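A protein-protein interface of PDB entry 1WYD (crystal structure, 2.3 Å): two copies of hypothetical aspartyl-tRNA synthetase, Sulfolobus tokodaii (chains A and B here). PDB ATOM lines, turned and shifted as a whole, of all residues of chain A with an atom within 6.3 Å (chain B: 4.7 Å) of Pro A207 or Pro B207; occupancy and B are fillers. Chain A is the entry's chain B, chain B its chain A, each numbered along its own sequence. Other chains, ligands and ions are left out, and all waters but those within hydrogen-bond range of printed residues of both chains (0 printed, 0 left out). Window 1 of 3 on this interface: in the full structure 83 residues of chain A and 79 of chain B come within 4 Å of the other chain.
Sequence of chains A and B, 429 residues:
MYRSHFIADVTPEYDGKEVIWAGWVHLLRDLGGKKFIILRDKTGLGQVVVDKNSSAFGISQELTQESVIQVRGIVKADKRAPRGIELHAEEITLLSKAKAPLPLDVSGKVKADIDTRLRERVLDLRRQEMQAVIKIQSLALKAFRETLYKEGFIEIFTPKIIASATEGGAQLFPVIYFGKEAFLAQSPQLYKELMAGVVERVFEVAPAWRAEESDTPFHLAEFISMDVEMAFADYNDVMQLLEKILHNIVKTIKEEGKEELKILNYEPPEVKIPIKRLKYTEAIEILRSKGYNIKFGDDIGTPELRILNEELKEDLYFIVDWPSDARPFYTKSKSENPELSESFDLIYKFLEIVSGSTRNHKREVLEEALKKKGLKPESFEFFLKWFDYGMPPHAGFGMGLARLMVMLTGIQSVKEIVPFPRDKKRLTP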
ATOM      1  N   PHE A 157     -12.986  -3.166 -30.001  1.00  0.00           N
ATOM      2  CA  PHE A 157     -14.082  -3.207 -29.027  1.00  0.00           C
ATOM      3  C   PHE A 157     -13.521  -2.855 -27.630  1.00  0.00           C
ATOM      4  O   PHE A 157     -12.664  -3.582 -27.116  1.00  0.00           O
ATOM      5  CB  PHE A 157     -14.733  -4.583 -29.007  1.00  0.00           C
ATOM      6  CG  PHE A 157     -15.728  -4.783 -30.100  1.00  0.00           C
ATOM      7  CD1 PHE A 157     -15.474  -5.675 -31.119  1.00  0.00           C
ATOM      8  CD2 PHE A 157     -16.911  -4.051 -30.125  1.00  0.00           C
ATOM      9  CE1 PHE A 157     -16.402  -5.847 -32.148  1.00  0.00           C
ATOM     10  CE2 PHE A 157     -17.845  -4.210 -31.127  1.00  0.00           C
ATOM     11  CZ  PHE A 157     -17.599  -5.112 -32.142  1.00  0.00           C
ATOM     12  N   THR A 158     -13.964  -1.712 -27.082  1.00  0.00           N
ATOM     13  CA  THR A 158     -13.488  -1.225 -25.808  1.00  0.00           C
ATOM     14  C   THR A 158     -14.538  -1.498 -24.679  1.00  0.00           C
ATOM     15  O   THR A 158     -15.709  -1.848 -24.962  1.00  0.00           O
ATOM     16  CB  THR A 158     -13.105   0.232 -25.870  1.00  0.00           C
ATOM     17  OG1 THR A 158     -14.165   0.973 -26.467  1.00  0.00           O
ATOM     18  CG2 THR A 158     -11.940   0.424 -26.802  1.00  0.00           C
ATOM     19  N   LYS A 160     -17.346  -1.486 -21.994  1.00  0.00           N
ATOM     20  CA  LYS A 160     -18.559  -0.713 -21.864  1.00  0.00           C
ATOM     21  C   LYS A 160     -18.860  -0.402 -20.382  1.00  0.00           C
ATOM     22  O   LYS A 160     -19.491   0.613 -20.082  1.00  0.00           O
ATOM     23  CB  LYS A 160     -19.735  -1.423 -22.548  1.00  0.00           C
ATOM     24  CG  LYS A 160     -19.574  -1.656 -24.052  1.00  0.00           C
ATOM     25  CD  LYS A 160     -19.156  -0.368 -24.733  1.00  0.00           C
ATOM     26  CE  LYS A 160     -18.520  -0.606 -26.064  1.00  0.00           C
ATOM     27  NZ  LYS A 160     -17.986   0.625 -26.611  1.00  0.00           N
ATOM     28  N   ALA A 185     -20.393   3.170 -20.049  1.00  0.00           N
ATOM     29  CA  ALA A 185     -19.632   4.173 -20.811  1.00  0.00           C
ATOM     30  C   ALA A 185     -20.515   5.051 -21.682  1.00  0.00           C
ATOM     31  O   ALA A 185     -21.501   4.584 -22.216  1.00  0.00           O
ATOM     32  CB  ALA A 185     -18.588   3.472 -21.665  1.00  0.00           C
ATOM     33  N   SER A 187     -19.002   6.699 -24.288  1.00  0.00           N
ATOM     34  CA  SER A 187     -18.264   6.822 -25.530  1.00  0.00           C
ATOM     35  C   SER A 187     -17.006   6.023 -25.309  1.00  0.00           C
ATOM     36  O   SER A 187     -16.660   5.796 -24.159  1.00  0.00           O
ATOM     37  CB  SER A 187     -17.967   8.286 -25.802  1.00  0.00           C
ATOM     38  OG  SER A 187     -16.607   8.608 -25.578  1.00  0.00           O
ATOM     39  N   GLU A 204     -14.512   1.990 -33.905  1.00  0.00           N
ATOM     40  CA  GLU A 204     -15.460   1.115 -33.267  1.00  0.00           C
ATOM     41  C   GLU A 204     -16.882   1.593 -33.545  1.00  0.00           C
ATOM     42  O   GLU A 204     -17.176   2.782 -33.514  1.00  0.00           O
ATOM     43  CB  GLU A 204     -15.095   1.043 -31.771  1.00  0.00           C
ATOM     44  CG  GLU A 204     -16.229   0.766 -30.801  1.00  0.00           C
ATOM     45  CD  GLU A 204     -15.761   0.280 -29.434  1.00  0.00           C
ATOM     46  OE1 GLU A 204     -14.819   0.852 -28.861  1.00  0.00           O
ATOM     47  OE2 GLU A 204     -16.351  -0.662 -28.921  1.00  0.00           O
ATOM     48  N   VAL A 205     -17.763   0.668 -33.862  1.00  0.00           N
ATOM     49  CA  VAL A 205     -19.179   0.970 -33.960  1.00  0.00           C
ATOM     50  C   VAL A 205     -19.781   0.122 -32.822  1.00  0.00           C
ATOM     51  O   VAL A 205     -19.610  -1.099 -32.815  1.00  0.00           O
ATOM     52  CB  VAL A 205     -19.783   0.496 -35.308  1.00  0.00           C
ATOM     53  CG1 VAL A 205     -21.178   1.001 -35.475  1.00  0.00           C
ATOM     54  CG2 VAL A 205     -18.963   0.981 -36.499  1.00  0.00           C
ATOM     55  N   ALA A 206     -20.481   0.748 -31.883  1.00  0.00           N
ATOM     56  CA  ALA A 206     -20.917   0.001 -30.681  1.00  0.00           C
ATOM     57  C   ALA A 206     -21.844   0.829 -29.817  1.00  0.00           C
ATOM     58  O   ALA A 206     -21.857   2.069 -29.920  1.00  0.00           O
ATOM     59  CB  ALA A 206     -19.728  -0.410 -29.881  1.00  0.00           C
ATOM     60  N   PRO A 207     -22.589   0.166 -28.919  1.00  0.00           N
ATOM     61  CA  PRO A 207     -23.501   0.889 -28.036  1.00  0.00           C
ATOM     62  C   PRO A 207     -22.740   1.818 -27.087  1.00  0.00           C
ATOM     63  O   PRO A 207     -21.598   1.551 -26.716  1.00  0.00           O
ATOM     64  CB  PRO A 207     -24.215  -0.242 -27.297  1.00  0.00           C
ATOM     65  CG  PRO A 207     -23.893  -1.505 -28.169  1.00  0.00           C
ATOM     66  CD  PRO A 207     -22.566  -1.277 -28.632  1.00  0.00           C
ATOM     67  N   ALA A 208     -23.372   2.950 -26.774  1.00  0.00           N
ATOM     68  CA  ALA A 208     -23.041   3.786 -25.625  1.00  0.00           C
ATOM     69  C   ALA A 208     -24.339   4.268 -24.866  1.00  0.00           C
ATOM     70  O   ALA A 208     -25.494   4.026 -25.274  1.00  0.00           O
ATOM     71  CB  ALA A 208     -22.233   4.973 -26.068  1.00  0.00           C
ATOM     72  N   TRP A 209     -24.156   4.960 -23.750  1.00  0.00           N
ATOM     73  CA  TRP A 209     -25.333   5.299 -22.942  1.00  0.00           C
ATOM     74  C   TRP A 209     -25.207   6.589 -22.164  1.00  0.00           C
ATOM     75  O   TRP A 209     -24.145   6.938 -21.660  1.00  0.00           O
ATOM     76  CB  TRP A 209     -25.627   4.168 -21.981  1.00  0.00           C
ATOM     77  CG  TRP A 209     -25.874   2.803 -22.584  1.00  0.00           C
ATOM     78  CD1 TRP A 209     -27.081   2.272 -22.939  1.00  0.00           C
ATOM     79  CD2 TRP A 209     -24.925   1.769 -22.751  1.00  0.00           C
ATOM     80  NE1 TRP A 209     -26.936   0.961 -23.340  1.00  0.00           N
ATOM     81  CE2 TRP A 209     -25.608   0.635 -23.243  1.00  0.00           C
ATOM     82  CE3 TRP A 209     -23.544   1.678 -22.546  1.00  0.00           C
ATOM     83  CZ2 TRP A 209     -24.956  -0.565 -23.561  1.00  0.00           C
ATOM     84  CZ3 TRP A 209     -22.899   0.475 -22.842  1.00  0.00           C
ATOM     85  CH2 TRP A 209     -23.607  -0.636 -23.329  1.00  0.00           C
ATOM     86  N   GLU A 222     -29.918   4.886 -24.722  1.00  0.00           N
ATOM     87  CA  GLU A 222     -29.019   3.983 -25.444  1.00  0.00           C
ATOM     88  C   GLU A 222     -28.864   4.359 -26.942  1.00  0.00           C
ATOM     89  O   GLU A 222     -29.831   4.640 -27.629  1.00  0.00           O
ATOM     90  CB  GLU A 222     -29.551   2.581 -25.375  1.00  0.00           C
ATOM     91  CG  GLU A 222     -28.528   1.530 -25.785  1.00  0.00           C
ATOM     92  CD  GLU A 222     -29.129   0.155 -25.625  1.00  0.00           C
ATOM     93  OE1 GLU A 222     -29.213  -0.328 -24.462  1.00  0.00           O
ATOM     94  OE2 GLU A 222     -29.578  -0.389 -26.656  1.00  0.00           O
ATOM     95  N   PHE A 223     -27.642   4.281 -27.450  1.00  0.00           N
ATOM     96  CA  PHE A 223     -27.374   4.752 -28.801  1.00  0.00           C
ATOM     97  C   PHE A 223     -26.086   4.155 -29.350  1.00  0.00           C
ATOM     98  O   PHE A 223     -25.150   3.923 -28.600  1.00  0.00           O
ATOM     99  CB  PHE A 223     -27.335   6.290 -28.856  1.00  0.00           C
ATOM    100  CG  PHE A 223     -26.438   6.942 -27.820  1.00  0.00           C
ATOM    101  CD1 PHE A 223     -25.093   7.233 -28.103  1.00  0.00           C
ATOM    102  CD2 PHE A 223     -26.960   7.339 -26.570  1.00  0.00           C
ATOM    103  CE1 PHE A 223     -24.270   7.862 -27.151  1.00  0.00           C
ATOM    104  CE2 PHE A 223     -26.133   7.964 -25.593  1.00  0.00           C
ATOM    105  CZ  PHE A 223     -24.799   8.220 -25.887  1.00  0.00           C
ATOM    106  N   ILE A 224     -26.052   3.930 -30.657  1.00  0.00           N
ATOM    107  CA  ILE A 224     -24.858   3.432 -31.331  1.00  0.00           C
ATOM    108  C   ILE A 224     -23.964   4.560 -31.796  1.00  0.00           C
ATOM    109  O   ILE A 224     -24.405   5.482 -32.465  1.00  0.00           O
ATOM    110  CB  ILE A 224     -25.277   2.566 -32.549  1.00  0.00           C
ATOM    111  CG1 ILE A 224     -26.275   1.482 -32.081  1.00  0.00           C
ATOM    112  CG2 ILE A 224     -24.063   2.020 -33.285  1.00  0.00           C
ATOM    113  CD1 ILE A 224     -25.696   0.474 -31.162  1.00  0.00           C
ATOM    114  N   SER A 225     -22.697   4.477 -31.424  1.00  0.00           N
ATOM    115  CA  SER A 225     -21.725   5.496 -31.688  1.00  0.00           C
ATOM    116  C   SER A 225     -20.702   4.891 -32.673  1.00  0.00           C
ATOM    117  O   SER A 225     -20.308   3.722 -32.547  1.00  0.00           O
ATOM    118  CB  SER A 225     -21.116   5.924 -30.346  1.00  0.00           C
ATOM    119  OG  SER A 225     -19.979   6.788 -30.450  1.00  0.00           O
ATOM    120  N   LYS B 160     -29.393  -3.277 -25.283  1.00  0.00           N
ATOM    121  CA  LYS B 160     -28.484  -3.831 -24.311  1.00  0.00           C
ATOM    122  C   LYS B 160     -29.040  -3.797 -22.883  1.00  0.00           C
ATOM    123  O   LYS B 160     -28.713  -4.666 -22.088  1.00  0.00           O
ATOM    124  CB  LYS B 160     -27.164  -3.081 -24.377  1.00  0.00           C
ATOM    125  CG  LYS B 160     -26.446  -3.207 -25.728  1.00  0.00           C
ATOM    126  CD  LYS B 160     -26.522  -4.678 -26.259  1.00  0.00           C
ATOM    127  CE  LYS B 160     -26.288  -4.724 -27.775  1.00  0.00           C
ATOM    128  NZ  LYS B 160     -26.834  -5.940 -28.421  1.00  0.00           N
ATOM    129  N   ALA B 206     -21.612  -7.362 -31.088  1.00  0.00           N
ATOM    130  CA  ALA B 206     -21.849  -6.404 -30.055  1.00  0.00           C
ATOM    131  C   ALA B 206     -21.600  -7.039 -28.632  1.00  0.00           C
ATOM    132  O   ALA B 206     -21.548  -8.294 -28.482  1.00  0.00           O
ATOM    133  CB  ALA B 206     -23.299  -5.882 -30.221  1.00  0.00           C
ATOM    134  N   PRO B 207     -21.373  -6.175 -27.638  1.00  0.00           N
ATOM    135  CA  PRO B 207     -21.083  -6.621 -26.257  1.00  0.00           C
ATOM    136  C   PRO B 207     -22.283  -7.258 -25.628  1.00  0.00           C
ATOM    137  O   PRO B 207     -23.422  -6.912 -25.904  1.00  0.00           O
ATOM    138  CB  PRO B 207     -20.784  -5.316 -25.508  1.00  0.00           C
ATOM    139  CG  PRO B 207     -20.485  -4.277 -26.649  1.00  0.00           C
ATOM    140  CD  PRO B 207     -21.365  -4.703 -27.775  1.00  0.00           C
ATOM    141  N   ALA B 208     -22.000  -8.222 -24.779  1.00  0.00           N
ATOM    142  CA  ALA B 208     -22.982  -8.851 -23.894  1.00  0.00           C
ATOM    143  C   ALA B 208     -22.308  -9.073 -22.540  1.00  0.00           C
ATOM    144  O   ALA B 208     -21.091  -8.970 -22.429  1.00  0.00           O
ATOM    145  CB  ALA B 208     -23.413 -10.177 -24.504  1.00  0.00           C
ATOM    146  N   TRP B 209     -23.084  -9.433 -21.516  1.00  0.00           N
ATOM    147  CA  TRP B 209     -22.565  -9.539 -20.155  1.00  0.00           C
ATOM    148  C   TRP B 209     -23.219 -10.693 -19.393  1.00  0.00           C
ATOM    149  O   TRP B 209     -24.409 -10.969 -19.529  1.00  0.00           O
ATOM    150  CB  TRP B 209     -22.770  -8.214 -19.379  1.00  0.00           C
ATOM    151  CG  TRP B 209     -22.266  -6.958 -20.100  1.00  0.00           C
ATOM    152  CD1 TRP B 209     -21.086  -6.319 -19.892  1.00  0.00           C
ATOM    153  CD2 TRP B 209     -22.933  -6.236 -21.137  1.00  0.00           C
ATOM    154  NE1 TRP B 209     -20.972  -5.233 -20.730  1.00  0.00           N
ATOM    155  CE2 TRP B 209     -22.098  -5.168 -21.513  1.00  0.00           C
ATOM    156  CE3 TRP B 209     -24.169  -6.387 -21.805  1.00  0.00           C
ATOM    157  CZ2 TRP B 209     -22.452  -4.258 -22.512  1.00  0.00           C
ATOM    158  CZ3 TRP B 209     -24.506  -5.490 -22.792  1.00  0.00           C
ATOM    159  CH2 TRP B 209     -23.662  -4.435 -23.135  1.00  0.00           C
ATOM    160  N   PHE B 223     -18.243  -9.606 -22.959  1.00  0.00           N
ATOM    161  CA  PHE B 223     -17.669 -10.301 -24.097  1.00  0.00           C
ATOM    162  C   PHE B 223     -18.340  -9.864 -25.389  1.00  0.00           C
ATOM    163  O   PHE B 223     -19.542  -9.528 -25.400  1.00  0.00           O
ATOM    164  CB  PHE B 223     -17.759 -11.807 -23.920  1.00  0.00           C
ATOM    165  CG  PHE B 223     -19.096 -12.271 -23.524  1.00  0.00           C
ATOM    166  CD1 PHE B 223     -20.021 -12.608 -24.483  1.00  0.00           C
ATOM    167  CD2 PHE B 223     -19.460 -12.347 -22.152  1.00  0.00           C
ATOM    168  CE1 PHE B 223     -21.275 -13.024 -24.133  1.00  0.00           C
ATOM    169  CE2 PHE B 223     -20.732 -12.741 -21.788  1.00  0.00           C
ATOM    170  CZ  PHE B 223     -21.635 -13.109 -22.769  1.00  0.00           C
ATOM    171  N   ILE B 224     -17.565  -9.856 -26.466  1.00  0.00           N
ATOM    172  CA  ILE B 224     -18.137  -9.553 -27.803  1.00  0.00           C
ATOM    173  C   ILE B 224     -18.667 -10.795 -28.485  1.00  0.00           C
ATOM    174  O   ILE B 224     -17.979 -11.799 -28.610  1.00  0.00           O
ATOM    175  CB  ILE B 224     -17.122  -8.860 -28.632  1.00  0.00           C
ATOM    176  CG1 ILE B 224     -16.627  -7.651 -27.842  1.00  0.00           C
ATOM    177  CG2 ILE B 224     -17.678  -8.519 -30.057  1.00  0.00           C
ATOM    178  CD1 ILE B 224     -17.595  -6.488 -27.786  1.00  0.00           C
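Of chain B, only Lys B160 and Pro B207 come within 4 Å of Pro A207. Pro B207 touches just these residues of chain A: Lys A160 (3.8 Å) and Pro A207 (3.7 Å). Printed residues of chain B within 4 Å of Glu A222: Lys B160 (3.1 Å). Of the printed residues of chain A, Lys B160 touches Pro A207, Trp A209 and Glu A222. Of the printed residues of chain A, Trp B209 touches Lys A160 and Trp A209. Of the printed residues of chain A, Ile B224 touches Phe A157 (3.4 Å). The nearest printed residue of chain B that does not touch Pro A207 is Ala B206 (4.9 Å). The nearest residue of chain A that does not touch Pro B207 is Phe A157 (4.9 Å). The nearest printed residue of chain A that does not touch Lys B160 is Ile A224 (6.2 Å).
Phe A157 touches Ile B224. Pro B207 touches Lys A160. CZ2 of Trp B209 touches CB of Lys A160 (3.9 Å). Pro A207 touches Lys B160. Pro B207 touches Pro A207. CZ2 of Trp A209 touches CB of Lys B160, 3.4 Å away. Trp A209 touches Trp B209.
Lys A160 touches Pro B207, and with the chains exchanged Pro A207 touches Lys B160. Lys A160 touches Trp B209, and with the chains exchanged Trp A209 touches Lys B160. Pro A207 touches its own counterpart, Pro B207. Trp B209 touches its own counterpart, Trp A209. Of the 8 pairs that touch across the chains among the printed residues, 6 have their exchanged pair printed and touching as well.
Of the 15 printed residues of chain A, 5 touch a printed residue of chain B. Hydrophobic or aromatic side chains of chain A that line the printed part of chain B: Phe A157, Pro A207 and Trp A209. Along chain A the printed residues that touch a printed residue of chain B span positions 157 to 222. Printed residues of chain B that touch a printed residue of chain A: Lys B160, Pro B207, Trp B209 and Ile B224. Hydrophobic or aromatic side chains of chain B that line the printed part of chain A: Pro B207, Trp B209 and Ile B224. Along chain B the printed residues that touch a printed residue of chain A span positions 160 to 224. Among the printed residues, 8 pairs touch across the chains.
The backbone NH of Lys B160 lies within hydrogen-bond range of the side-chain carboxylate of Glu A222 (3.1 Å).
The backbone carbonyl oxygen (O) of Lys A160 sits at hydrogen-bond distance from the backbone NH (N) of Ala A185. The side-chain amino group (NZ) of Lys A160 is in salt-bridge range of the side-chain carboxylate (OE2) of Glu A204. The backbone NH (N) of Trp A209 sits at hydrogen-bond distance from the backbone carbonyl oxygen (O) of Ala A185 (3.1 Å). The side-chain carboxylate (OE1) of Glu A222 is in hydrogen-bond range of the indole nitrogen (NE1) of Trp A209 (2.8 Å).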
